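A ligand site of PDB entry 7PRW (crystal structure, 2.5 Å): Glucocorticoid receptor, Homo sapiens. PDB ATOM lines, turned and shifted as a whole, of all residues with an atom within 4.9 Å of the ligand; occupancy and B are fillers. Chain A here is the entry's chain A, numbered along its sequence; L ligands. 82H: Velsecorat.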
ATOM      1  N   GLU A 156      14.007 -13.599  38.757  1.00  0.00           N
ATOM      2  CA  GLU A 156      13.707 -13.007  37.473  1.00  0.00           C
ATOM      3  C   GLU A 156      14.433 -13.792  36.379  1.00  0.00           C
ATOM      4  O   GLU A 156      15.651 -14.034  36.495  1.00  0.00           O
ATOM      5  CB  GLU A 156      14.091 -11.521  37.465  1.00  0.00           C
ATOM      6  CG  GLU A 156      13.688 -10.769  36.207  1.00  0.00           C
ATOM      7  CD  GLU A 156      12.232 -10.856  35.797  1.00  0.00           C
ATOM      8  OE1 GLU A 156      11.370 -11.123  36.676  1.00  0.00           O
ATOM      9  OE2 GLU A 156      11.945 -10.637  34.602  1.00  0.00           O
ATOM     10  N   PRO A 157      13.676 -14.279  35.351  1.00  0.00           N
ATOM     11  CA  PRO A 157      14.294 -15.082  34.289  1.00  0.00           C
ATOM     12  C   PRO A 157      15.451 -14.391  33.592  1.00  0.00           C
ATOM     13  O   PRO A 157      15.516 -13.150  33.538  1.00  0.00           O
ATOM     14  CB  PRO A 157      13.138 -15.351  33.319  1.00  0.00           C
ATOM     15  CG  PRO A 157      11.925 -15.239  34.148  1.00  0.00           C
ATOM     16  CD  PRO A 157      12.219 -14.131  35.127  1.00  0.00           C
ATOM     17  N   MET A 176       8.800 -14.051  12.524  1.00  0.00           N
ATOM     18  CA  MET A 176       7.719 -14.523  13.385  1.00  0.00           C
ATOM     19  C   MET A 176       7.937 -15.931  13.864  1.00  0.00           C
ATOM     20  O   MET A 176       7.573 -16.243  14.999  1.00  0.00           O
ATOM     21  CB  MET A 176       6.364 -14.434  12.697  1.00  0.00           C
ATOM     22  CG  MET A 176       5.539 -13.311  13.197  1.00  0.00           C
ATOM     23  SD  MET A 176       4.333 -12.856  11.934  1.00  0.00           S
ATOM     24  CE  MET A 176       4.146 -11.150  12.310  1.00  0.00           C
ATOM     25  N   LEU A 179      10.620 -15.814  16.628  1.00  0.00           N
ATOM     26  CA  LEU A 179      10.048 -15.260  17.847  1.00  0.00           C
ATOM     27  C   LEU A 179       9.041 -16.170  18.531  1.00  0.00           C
ATOM     28  O   LEU A 179       8.892 -16.097  19.746  1.00  0.00           O
ATOM     29  CB  LEU A 179       9.443 -13.875  17.597  1.00  0.00           C
ATOM     30  CG  LEU A 179      10.403 -12.845  17.095  1.00  0.00           C
ATOM     31  CD1 LEU A 179       9.673 -11.604  16.674  1.00  0.00           C
ATOM     32  CD2 LEU A 179      11.470 -12.554  18.104  1.00  0.00           C
ATOM     33  N   ASN A 180       8.371 -17.034  17.768  1.00  0.00           N
ATOM     34  CA  ASN A 180       7.452 -17.999  18.364  1.00  0.00           C
ATOM     35  C   ASN A 180       8.278 -19.085  19.032  1.00  0.00           C
ATOM     36  O   ASN A 180       8.011 -19.402  20.187  1.00  0.00           O
ATOM     37  CB  ASN A 180       6.519 -18.568  17.319  1.00  0.00           C
ATOM     38  CG  ASN A 180       5.435 -17.618  16.910  1.00  0.00           C
ATOM     39  OD1 ASN A 180       5.151 -16.634  17.569  1.00  0.00           O
ATOM     40  ND2 ASN A 180       4.800 -17.876  15.790  1.00  0.00           N
ATOM     41  N   LEU A 182      11.270 -18.734  20.143  1.00  0.00           N
ATOM     42  CA  LEU A 182      11.928 -18.088  21.272  1.00  0.00           C
ATOM     43  C   LEU A 182      10.913 -17.943  22.403  1.00  0.00           C
ATOM     44  O   LEU A 182      11.216 -18.286  23.533  1.00  0.00           O
ATOM     45  CB  LEU A 182      12.478 -16.697  20.875  1.00  0.00           C
ATOM     46  CG  LEU A 182      12.985 -15.815  22.022  1.00  0.00           C
ATOM     47  CD1 LEU A 182      14.212 -16.416  22.667  1.00  0.00           C
ATOM     48  CD2 LEU A 182      13.249 -14.390  21.551  1.00  0.00           C
ATOM     49  N   GLY A 183       9.718 -17.456  22.073  1.00  0.00           N
ATOM     50  CA  GLY A 183       8.614 -17.292  23.003  1.00  0.00           C
ATOM     51  C   GLY A 183       8.236 -18.568  23.728  1.00  0.00           C
ATOM     52  O   GLY A 183       7.792 -18.525  24.876  1.00  0.00           O
ATOM     53  N   GLN A 186      10.839 -18.814  26.407  1.00  0.00           N
ATOM     54  CA  GLN A 186      10.539 -17.766  27.395  1.00  0.00           C
ATOM     55  C   GLN A 186       9.392 -18.262  28.288  1.00  0.00           C
ATOM     56  O   GLN A 186       9.431 -18.046  29.505  1.00  0.00           O
ATOM     57  CB  GLN A 186      10.164 -16.417  26.743  1.00  0.00           C
ATOM     58  CG  GLN A 186      11.298 -15.743  25.956  1.00  0.00           C
ATOM     59  CD  GLN A 186      12.329 -14.958  26.767  1.00  0.00           C
ATOM     60  OE1 GLN A 186      13.131 -14.183  26.203  1.00  0.00           O
ATOM     61  NE2 GLN A 186      12.363 -15.135  28.095  1.00  0.00           N
ATOM     62  N   ALA A 190       9.049 -18.819  32.241  1.00  0.00           N
ATOM     63  CA  ALA A 190       7.891 -18.236  32.907  1.00  0.00           C
ATOM     64  C   ALA A 190       7.153 -19.248  33.791  1.00  0.00           C
ATOM     65  O   ALA A 190       6.444 -18.853  34.706  1.00  0.00           O
ATOM     66  CB  ALA A 190       6.929 -17.639  31.881  1.00  0.00           C
ATOM     67  N   TRP A 193       9.530 -19.664  36.868  1.00  0.00           N
ATOM     68  CA  TRP A 193       9.437 -18.398  37.585  1.00  0.00           C
ATOM     69  C   TRP A 193       8.191 -18.463  38.463  1.00  0.00           C
ATOM     70  O   TRP A 193       8.281 -18.222  39.662  1.00  0.00           O
ATOM     71  CB  TRP A 193       9.381 -17.224  36.586  1.00  0.00           C
ATOM     72  CG  TRP A 193       9.046 -15.895  37.181  1.00  0.00           C
ATOM     73  CD1 TRP A 193       9.884 -15.063  37.869  1.00  0.00           C
ATOM     74  CD2 TRP A 193       7.793 -15.199  37.078  1.00  0.00           C
ATOM     75  NE1 TRP A 193       9.220 -13.910  38.217  1.00  0.00           N
ATOM     76  CE2 TRP A 193       7.926 -13.982  37.770  1.00  0.00           C
ATOM     77  CE3 TRP A 193       6.563 -15.515  36.506  1.00  0.00           C
ATOM     78  CZ2 TRP A 193       6.874 -13.074  37.889  1.00  0.00           C
ATOM     79  CZ3 TRP A 193       5.519 -14.617  36.621  1.00  0.00           C
ATOM     80  CH2 TRP A 193       5.685 -13.411  37.312  1.00  0.00           C
ATOM     81  N   TRP A 216      -0.286 -15.754  30.061  1.00  0.00           N
ATOM     82  CA  TRP A 216       1.029 -15.883  29.428  1.00  0.00           C
ATOM     83  C   TRP A 216       1.395 -14.708  28.554  1.00  0.00           C
ATOM     84  O   TRP A 216       2.567 -14.341  28.495  1.00  0.00           O
ATOM     85  CB  TRP A 216       1.155 -17.183  28.634  1.00  0.00           C
ATOM     86  CG  TRP A 216       0.308 -17.257  27.398  1.00  0.00           C
ATOM     87  CD1 TRP A 216      -0.966 -17.741  27.313  1.00  0.00           C
ATOM     88  CD2 TRP A 216       0.709 -16.930  26.061  1.00  0.00           C
ATOM     89  NE1 TRP A 216      -1.404 -17.676  26.010  1.00  0.00           N
ATOM     90  CE2 TRP A 216      -0.385 -17.200  25.221  1.00  0.00           C
ATOM     91  CE3 TRP A 216       1.877 -16.411  25.507  1.00  0.00           C
ATOM     92  CZ2 TRP A 216      -0.347 -16.981  23.845  1.00  0.00           C
ATOM     93  CZ3 TRP A 216       1.919 -16.183  24.142  1.00  0.00           C
ATOM     94  CH2 TRP A 216       0.827 -16.486  23.328  1.00  0.00           C
ATOM     95  N   MET A 217       0.410 -14.124  27.882  1.00  0.00           N
ATOM     96  CA  MET A 217       0.657 -12.978  27.013  1.00  0.00           C
ATOM     97  C   MET A 217       0.845 -11.684  27.803  1.00  0.00           C
ATOM     98  O   MET A 217       1.544 -10.796  27.331  1.00  0.00           O
ATOM     99  CB  MET A 217      -0.416 -12.841  25.934  1.00  0.00           C
ATOM    100  CG  MET A 217      -0.071 -11.843  24.862  1.00  0.00           C
ATOM    101  SD  MET A 217       1.432 -12.299  24.000  1.00  0.00           S
ATOM    102  CE  MET A 217       0.742 -13.004  22.527  1.00  0.00           C
ATOM    103  N   LEU A 219       2.435 -11.560  30.769  1.00  0.00           N
ATOM    104  CA  LEU A 219       3.804 -11.753  31.226  1.00  0.00           C
ATOM    105  C   LEU A 219       4.838 -11.555  30.095  1.00  0.00           C
ATOM    106  O   LEU A 219       5.898 -10.991  30.344  1.00  0.00           O
ATOM    107  CB  LEU A 219       3.976 -13.156  31.846  1.00  0.00           C
ATOM    108  CG  LEU A 219       3.011 -13.491  32.972  1.00  0.00           C
ATOM    109  CD1 LEU A 219       3.027 -14.966  33.279  1.00  0.00           C
ATOM    110  CD2 LEU A 219       3.327 -12.701  34.218  1.00  0.00           C
ATOM    111  N   MET A 220       4.519 -11.999  28.871  1.00  0.00           N
ATOM    112  CA  MET A 220       5.461 -11.842  27.765  1.00  0.00           C
ATOM    113  C   MET A 220       5.513 -10.421  27.226  1.00  0.00           C
ATOM    114  O   MET A 220       6.600  -9.907  27.039  1.00  0.00           O
ATOM    115  CB  MET A 220       5.203 -12.862  26.675  1.00  0.00           C
ATOM    116  CG  MET A 220       5.596 -14.248  27.098  1.00  0.00           C
ATOM    117  SD  MET A 220       5.759 -15.424  25.735  1.00  0.00           S
ATOM    118  CE  MET A 220       5.283 -16.838  26.519  1.00  0.00           C
ATOM    119  N   ALA A 221       4.354  -9.762  27.056  1.00  0.00           N
ATOM    120  CA  ALA A 221       4.336  -8.363  26.594  1.00  0.00           C
ATOM    121  C   ALA A 221       4.801  -7.400  27.700  1.00  0.00           C
ATOM    122  O   ALA A 221       5.275  -6.317  27.378  1.00  0.00           O
ATOM    123  CB  ALA A 221       2.950  -7.965  26.109  1.00  0.00           C
ATOM    124  N   ALA A 223       7.221  -8.225  30.174  1.00  0.00           N
ATOM    125  CA  ALA A 223       8.673  -8.387  30.280  1.00  0.00           C
ATOM    126  C   ALA A 223       9.389  -7.919  29.026  1.00  0.00           C
ATOM    127  O   ALA A 223      10.540  -7.460  29.126  1.00  0.00           O
ATOM    128  CB  ALA A 223       9.036  -9.813  30.604  1.00  0.00           C
ATOM    129  N   LEU A 224       8.722  -8.011  27.849  1.00  0.00           N
ATOM    130  CA  LEU A 224       9.255  -7.524  26.583  1.00  0.00           C
ATOM    131  C   LEU A 224       9.225  -5.998  26.585  1.00  0.00           C
ATOM    132  O   LEU A 224      10.172  -5.383  26.102  1.00  0.00           O
ATOM    133  CB  LEU A 224       8.456  -8.038  25.386  1.00  0.00           C
ATOM    134  CG  LEU A 224       8.778  -7.401  24.031  1.00  0.00           C
ATOM    135  CD1 LEU A 224      10.091  -7.860  23.523  1.00  0.00           C
ATOM    136  CD2 LEU A 224       7.713  -7.654  23.056  1.00  0.00           C
ATOM    137  N   ARG A 227      12.038  -4.744  28.769  1.00  0.00           N
ATOM    138  CA  ARG A 227      13.330  -4.917  28.104  1.00  0.00           C
ATOM    139  C   ARG A 227      13.523  -3.905  26.967  1.00  0.00           C
ATOM    140  O   ARG A 227      14.633  -3.444  26.742  1.00  0.00           O
ATOM    141  CB  ARG A 227      13.549  -6.349  27.592  1.00  0.00           C
ATOM    142  CG  ARG A 227      15.039  -6.706  27.468  1.00  0.00           C
ATOM    143  CD  ARG A 227      15.264  -8.122  26.978  1.00  0.00           C
ATOM    144  NE  ARG A 227      14.716  -9.088  27.912  1.00  0.00           N
ATOM    145  CZ  ARG A 227      14.630 -10.400  27.693  1.00  0.00           C
ATOM    146  NH1 ARG A 227      14.097 -11.193  28.605  1.00  0.00           N
ATOM    147  NH2 ARG A 227      15.091 -10.916  26.554  1.00  0.00           N
ATOM    148  N   CYS A 238      12.804  -5.129  21.796  1.00  0.00           N
ATOM    149  CA  CYS A 238      13.983  -5.929  22.091  1.00  0.00           C
ATOM    150  C   CYS A 238      13.633  -7.324  22.492  1.00  0.00           C
ATOM    151  O   CYS A 238      13.766  -7.704  23.651  1.00  0.00           O
ATOM    152  CB  CYS A 238      14.851  -5.241  23.128  1.00  0.00           C
ATOM    153  SG  CYS A 238      15.301  -3.563  22.673  1.00  0.00           S
ATOM    154  N   PHE A 239      13.222  -8.128  21.512  1.00  0.00           N
ATOM    155  CA  PHE A 239      12.850  -9.511  21.752  1.00  0.00           C
ATOM    156  C   PHE A 239      14.010 -10.305  22.347  1.00  0.00           C
ATOM    157  O   PHE A 239      13.866 -10.942  23.392  1.00  0.00           O
ATOM    158  CB  PHE A 239      12.276 -10.140  20.469  1.00  0.00           C
ATOM    159  CG  PHE A 239      10.817  -9.809  20.211  1.00  0.00           C
ATOM    160  CD1 PHE A 239       9.812 -10.511  20.840  1.00  0.00           C
ATOM    161  CD2 PHE A 239      10.467  -8.802  19.330  1.00  0.00           C
ATOM    162  CE1 PHE A 239       8.475 -10.203  20.597  1.00  0.00           C
ATOM    163  CE2 PHE A 239       9.125  -8.495  19.109  1.00  0.00           C
ATOM    164  CZ  PHE A 239       8.143  -9.197  19.739  1.00  0.00           C
ATOM    165  N   MET A 255       3.769  -7.044  10.168  1.00  0.00           N
ATOM    166  CA  MET A 255       4.542  -6.770  11.370  1.00  0.00           C
ATOM    167  C   MET A 255       4.058  -5.570  12.174  1.00  0.00           C
ATOM    168  O   MET A 255       3.767  -5.731  13.351  1.00  0.00           O
ATOM    169  CB  MET A 255       6.038  -6.612  11.028  1.00  0.00           C
ATOM    170  CG  MET A 255       6.706  -7.908  10.653  1.00  0.00           C
ATOM    171  SD  MET A 255       7.145  -8.940  12.086  1.00  0.00           S
ATOM    172  CE  MET A 255       8.201  -7.821  12.977  1.00  0.00           C
ATOM    173  N   GLN A 258       1.113  -5.484  15.055  1.00  0.00           N
ATOM    174  CA  GLN A 258       1.356  -6.297  16.237  1.00  0.00           C
ATOM    175  C   GLN A 258       2.468  -5.694  17.103  1.00  0.00           C
ATOM    176  O   GLN A 258       2.346  -5.683  18.321  1.00  0.00           O
ATOM    177  CB  GLN A 258       1.665  -7.751  15.843  1.00  0.00           C
ATOM    178  CG  GLN A 258       1.824  -8.719  16.988  1.00  0.00           C
ATOM    179  CD  GLN A 258       0.550  -9.253  17.598  1.00  0.00           C
ATOM    180  OE1 GLN A 258      -0.502  -8.615  17.615  1.00  0.00           O
ATOM    181  NE2 GLN A 258       0.632 -10.457  18.116  1.00  0.00           N
ATOM    182  N   CYS A 259       3.497  -5.121  16.476  1.00  0.00           N
ATOM    183  CA  CYS A 259       4.607  -4.477  17.169  1.00  0.00           C
ATOM    184  C   CYS A 259       4.144  -3.264  17.918  1.00  0.00           C
ATOM    185  O   CYS A 259       4.607  -3.026  19.036  1.00  0.00           O
ATOM    186  CB  CYS A 259       5.742  -4.134  16.207  1.00  0.00           C
ATOM    187  SG  CYS A 259       6.483  -5.581  15.387  1.00  0.00           S
ATOM    188  N   MET A 262       2.929  -4.089  21.407  1.00  0.00           N
ATOM    189  CA  MET A 262       4.026  -4.379  22.330  1.00  0.00           C
ATOM    190  C   MET A 262       4.713  -3.068  22.739  1.00  0.00           C
ATOM    191  O   MET A 262       5.163  -2.928  23.873  1.00  0.00           O
ATOM    192  CB  MET A 262       5.066  -5.271  21.632  1.00  0.00           C
ATOM    193  CG  MET A 262       4.540  -6.588  21.194  1.00  0.00           C
ATOM    194  SD  MET A 262       4.194  -7.612  22.624  1.00  0.00           S
ATOM    195  CE  MET A 262       4.202  -9.225  21.849  1.00  0.00           C
ATOM    196  N   LYS A 283       4.482  -7.325  37.413  1.00  0.00           N
ATOM    197  CA  LYS A 283       4.565  -8.563  36.668  1.00  0.00           C
ATOM    198  C   LYS A 283       3.896  -9.709  37.412  1.00  0.00           C
ATOM    199  O   LYS A 283       3.024 -10.355  36.839  1.00  0.00           O
ATOM    200  CB  LYS A 283       6.004  -8.910  36.319  1.00  0.00           C
ATOM    201  CG  LYS A 283       6.091  -9.999  35.266  1.00  0.00           C
ATOM    202  CD  LYS A 283       7.318  -9.819  34.441  1.00  0.00           C
ATOM    203  CE  LYS A 283       8.543 -10.213  35.210  1.00  0.00           C
ATOM    204  NZ  LYS A 283       8.664 -11.680  35.272  1.00  0.00           N
ATOM    205  N   LEU A 348      -3.298  -8.440  21.256  1.00  0.00           N
ATOM    206  CA  LEU A 348      -2.168  -9.280  20.889  1.00  0.00           C
ATOM    207  C   LEU A 348      -2.658 -10.689  20.579  1.00  0.00           C
ATOM    208  O   LEU A 348      -2.227 -11.281  19.586  1.00  0.00           O
ATOM    209  CB  LEU A 348      -1.157  -9.338  22.037  1.00  0.00           C
ATOM    210  CG  LEU A 348      -0.373  -8.094  22.271  1.00  0.00           C
ATOM    211  CD1 LEU A 348       0.291  -8.160  23.604  1.00  0.00           C
ATOM    212  CD2 LEU A 348       0.633  -7.894  21.185  1.00  0.00           C
ATOM    213  N   TYR A 351      -4.633 -11.198  17.066  1.00  0.00           N
ATOM    214  CA  TYR A 351      -3.796 -11.407  15.886  1.00  0.00           C
ATOM    215  C   TYR A 351      -3.053 -12.752  15.956  1.00  0.00           C
ATOM    216  O   TYR A 351      -2.916 -13.433  14.943  1.00  0.00           O
ATOM    217  CB  TYR A 351      -2.812 -10.239  15.657  1.00  0.00           C
ATOM    218  CG  TYR A 351      -1.892 -10.476  14.473  1.00  0.00           C
ATOM    219  CD1 TYR A 351      -2.393 -10.584  13.189  1.00  0.00           C
ATOM    220  CD2 TYR A 351      -0.536 -10.702  14.671  1.00  0.00           C
ATOM    221  CE1 TYR A 351      -1.555 -10.862  12.120  1.00  0.00           C
ATOM    222  CE2 TYR A 351       0.310 -10.975  13.605  1.00  0.00           C
ATOM    223  CZ  TYR A 351      -0.199 -11.034  12.321  1.00  0.00           C
ATOM    224  OH  TYR A 351       0.623 -11.328  11.261  1.00  0.00           O
ATOM    225  N   CYS A 352      -2.587 -13.128  17.154  1.00  0.00           N
ATOM    226  CA  CYS A 352      -1.866 -14.376  17.331  1.00  0.00           C
ATOM    227  C   CYS A 352      -2.741 -15.566  16.989  1.00  0.00           C
ATOM    228  O   CYS A 352      -2.335 -16.428  16.230  1.00  0.00           O
ATOM    229  CB  CYS A 352      -1.313 -14.495  18.743  1.00  0.00           C
ATOM    230  SG  CYS A 352      -0.352 -16.004  19.033  1.00  0.00           S
ATOM    231  N   THR A 355      -3.430 -15.763  13.285  1.00  0.00           N
ATOM    232  CA  THR A 355      -2.242 -16.276  12.608  1.00  0.00           C
ATOM    233  C   THR A 355      -2.104 -17.764  12.784  1.00  0.00           C
ATOM    234  O   THR A 355      -1.831 -18.481  11.812  1.00  0.00           O
ATOM    235  CB  THR A 355      -1.020 -15.525  13.105  1.00  0.00           C
ATOM    236  OG1 THR A 355      -1.122 -14.205  12.603  1.00  0.00           O
ATOM    237  CG2 THR A 355       0.285 -16.161  12.648  1.00  0.00           C
ATOM    238  N   ILE A 363       2.958 -19.965   9.714  1.00  0.00           N
ATOM    239  CA  ILE A 363       4.077 -19.572  10.567  1.00  0.00           C
ATOM    240  C   ILE A 363       4.246 -20.660  11.656  1.00  0.00           C
ATOM    241  O   ILE A 363       3.260 -21.286  12.050  1.00  0.00           O
ATOM    242  CB  ILE A 363       3.843 -18.112  11.072  1.00  0.00           C
ATOM    243  CG1 ILE A 363       4.720 -17.122  10.310  1.00  0.00           C
ATOM    244  CG2 ILE A 363       3.991 -17.960  12.567  1.00  0.00           C
ATOM    245  CD1 ILE A 363       4.248 -16.809   8.941  1.00  0.00           C
ATOM    246  N   PHE A 365       4.800 -22.341  15.294  1.00  0.00           N
ATOM    247  CA  PHE A 365       4.600 -22.161  16.730  1.00  0.00           C
ATOM    248  C   PHE A 365       5.166 -23.423  17.417  1.00  0.00           C
ATOM    249  O   PHE A 365       4.964 -24.532  16.923  1.00  0.00           O
ATOM    250  CB  PHE A 365       3.104 -22.013  17.051  1.00  0.00           C
ATOM    251  CG  PHE A 365       2.488 -20.720  16.588  1.00  0.00           C
ATOM    252  CD1 PHE A 365       2.097 -20.536  15.277  1.00  0.00           C
ATOM    253  CD2 PHE A 365       2.272 -19.682  17.481  1.00  0.00           C
ATOM    254  CE1 PHE A 365       1.527 -19.349  14.856  1.00  0.00           C
ATOM    255  CE2 PHE A 365       1.677 -18.494  17.059  1.00  0.00           C
ATOM    256  CZ  PHE A 365       1.322 -18.329  15.751  1.00  0.00           C
ATOM    257  N   LEU A 369       3.851 -23.781  23.070  1.00  0.00           N
ATOM    258  CA  LEU A 369       2.979 -22.642  22.815  1.00  0.00           C
ATOM    259  C   LEU A 369       1.719 -23.000  22.062  1.00  0.00           C
ATOM    260  O   LEU A 369       0.650 -22.517  22.406  1.00  0.00           O
ATOM    261  CB  LEU A 369       3.723 -21.530  22.101  1.00  0.00           C
ATOM    262  CG  LEU A 369       4.075 -20.360  22.957  1.00  0.00           C
ATOM    263  CD1 LEU A 369       5.014 -19.443  22.233  1.00  0.00           C
ATOM    264  CD2 LEU A 369       2.838 -19.626  23.378  1.00  0.00           C
HETATM  265  C1  82H L   1      11.322 -10.665  26.410  1.00  0.00           C
HETATM  266  C2  82H L   1      10.884 -11.255  27.587  1.00  0.00           C
HETATM  267  C3  82H L   1       5.917 -13.481  17.774  1.00  0.00           C
HETATM  268  C7  82H L   1       5.849 -12.435  22.952  1.00  0.00           C
HETATM  269  C8  82H L   1       7.150 -13.903  21.546  1.00  0.00           C
HETATM  270  C9  82H L   1       9.392 -12.696  26.301  1.00  0.00           C
HETATM  271  C10 82H L   1       4.688 -11.762  18.918  1.00  0.00           C
HETATM  272  C11 82H L   1       9.653 -13.909  22.270  1.00  0.00           C
HETATM  273  C12 82H L   1       8.283 -13.563  22.308  1.00  0.00           C
HETATM  274  C13 82H L   1       9.912 -12.252  27.516  1.00  0.00           C
HETATM  275  C14 82H L   1       5.140 -13.081  18.866  1.00  0.00           C
HETATM  276  C15 82H L   1       8.177 -12.672  23.366  1.00  0.00           C
HETATM  277  C16 82H L   1       9.846 -12.095  25.129  1.00  0.00           C
HETATM  278  C19 82H L   1       5.920 -13.314  21.857  1.00  0.00           C
HETATM  279  C20 82H L   1       9.438 -12.899  28.731  1.00  0.00           C
HETATM  280  C21 82H L   1       2.299 -13.967  17.489  1.00  0.00           C
HETATM  281  C22 82H L   1       9.282 -14.849  31.066  1.00  0.00           C
HETATM  282  C24 82H L   1       5.460  -9.261  15.688  1.00  0.00           C
HETATM  283  C27 82H L   1      10.298 -13.717  30.977  1.00  0.00           C
HETATM  284  C30 82H L   1       4.823 -14.114  19.882  1.00  0.00           C
HETATM  285  C31 82H L   1       3.431 -14.641  19.579  1.00  0.00           C
HETATM  286  C32 82H L   1       2.365 -14.026  15.981  1.00  0.00           C
HETATM  287  C4  82H L   1       6.961 -12.086  23.722  1.00  0.00           C
HETATM  288  C5  82H L   1      10.803 -11.088  25.188  1.00  0.00           C
HETATM  289  C6  82H L   1       6.246 -12.639  16.730  1.00  0.00           C
HETATM  290  C17 82H L   1       5.806 -11.322  16.789  1.00  0.00           C
HETATM  291  C18 82H L   1       5.045 -10.891  17.879  1.00  0.00           C
HETATM  292  C23 82H L   1       8.247 -14.328  32.042  1.00  0.00           C
HETATM  293  C25 82H L   1       5.291  -8.662  17.077  1.00  0.00           C
HETATM  294  C26 82H L   1       9.925 -12.801  32.132  1.00  0.00           C
HETATM  295  C28 82H L   1       3.203 -15.887  20.400  1.00  0.00           C
HETATM  296  C29 82H L   1       2.833 -12.667  15.515  1.00  0.00           C
HETATM  297  N33 82H L   1      10.359 -13.292  23.219  1.00  0.00           N
HETATM  298  N34 82H L   1       9.447 -12.556  23.879  1.00  0.00           N
HETATM  299  N35 82H L   1      10.415 -13.032  29.708  1.00  0.00           N
HETATM  300  N36 82H L   1       3.109 -14.853  18.180  1.00  0.00           N
HETATM  301  O37 82H L   1       8.273 -13.260  28.754  1.00  0.00           O
HETATM  302  O38 82H L   1       1.592 -13.132  18.032  1.00  0.00           O
HETATM  303  O39 82H L   1       6.176 -10.507  15.754  1.00  0.00           O
HETATM  304  O40 82H L   1       4.612  -9.589  17.948  1.00  0.00           O
HETATM  305  O41 82H L   1       8.921 -13.437  32.941  1.00  0.00           O
HETATM  306  O42 82H L   1       4.729 -13.550  21.181  1.00  0.00           O
HETATM  307  F43 82H L   1       3.204 -14.980  15.473  1.00  0.00           F
HETATM  308  F44 82H L   1       1.130 -14.214  15.431  1.00  0.00           F
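Merely in contact with the ligand: Glu 156 (3.9 Å), Pro 157 (3.7 Å), Met 176 (3.6 Å), Leu 179 (3.3 Å), Leu 182 (3.5 Å), Gly 183 (3.6 Å), Ala 190 (3.6 Å), Trp 216 (3.8 Å), Leu 219 (3.6 Å), Met 220 (3.3 Å), Ala 223 (3.5 Å), Leu 224 (3.7 Å), Arg 227 (3.4 Å), Phe 239 (3.6 Å), Met 255 (3.99 Å), Cys 259 (3.7 Å), Met 262 (3.8 Å), Tyr 351 (3.6 Å), Thr 355 (3.4 Å) and Phe 365 (3.9 Å). Hydrophobic or aromatic side chains within 4 Å of the ligand: Pro 157, Met 176, Leu 179, Leu 182, Ala 190, Trp 216, Met 220, Ala 223, Leu 224, Phe 239, Met 255, Met 262, Tyr 351 and Phe 365. The nearest printed residue that does not touch the ligand is Ile 363 (4.2 Å).
An oxygen (O38) of the ligand is in hydrogen-bond range of the side-chain amide nitrogen of Gln 258, 2.8 Å away. O41 of the ligand lies within hydrogen-bond range of NZ of Lys 283, 2.9 Å away. NE2 of Gln 186 lies close to N35 of the ligand, at 3.3 Å. An oxygen (O38) of the ligand lies close to the side-chain sulfur (SG) of Cys 352, 3.6 Å away. OD1 of Asn 180 lies within hydrogen-bond range of N36 of the ligand, at 2.8 Å.
NH2 of Arg 227 sits at hydrogen-bond distance from O of Phe 239 (3.4 Å). The side-chain amide nitrogen of Asn 180 sits close to the backbone carbonyl oxygen of Met 176 (3.3 Å). O of Leu 348 sits at hydrogen-bond distance from NE2 of Gln 258, 3.3 Å away. The side-chain hydroxyl of Thr 355 lies within hydrogen-bond range of the backbone carbonyl oxygen of Tyr 351. The side-chain amino group (NZ) of Lys 283 is in salt-bridge range of the side-chain carboxylate (OE1) of Glu 156 (3.1 Å). SG of Cys 259 sits at hydrogen-bond distance from O of Met 255, 3.4 Å away.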
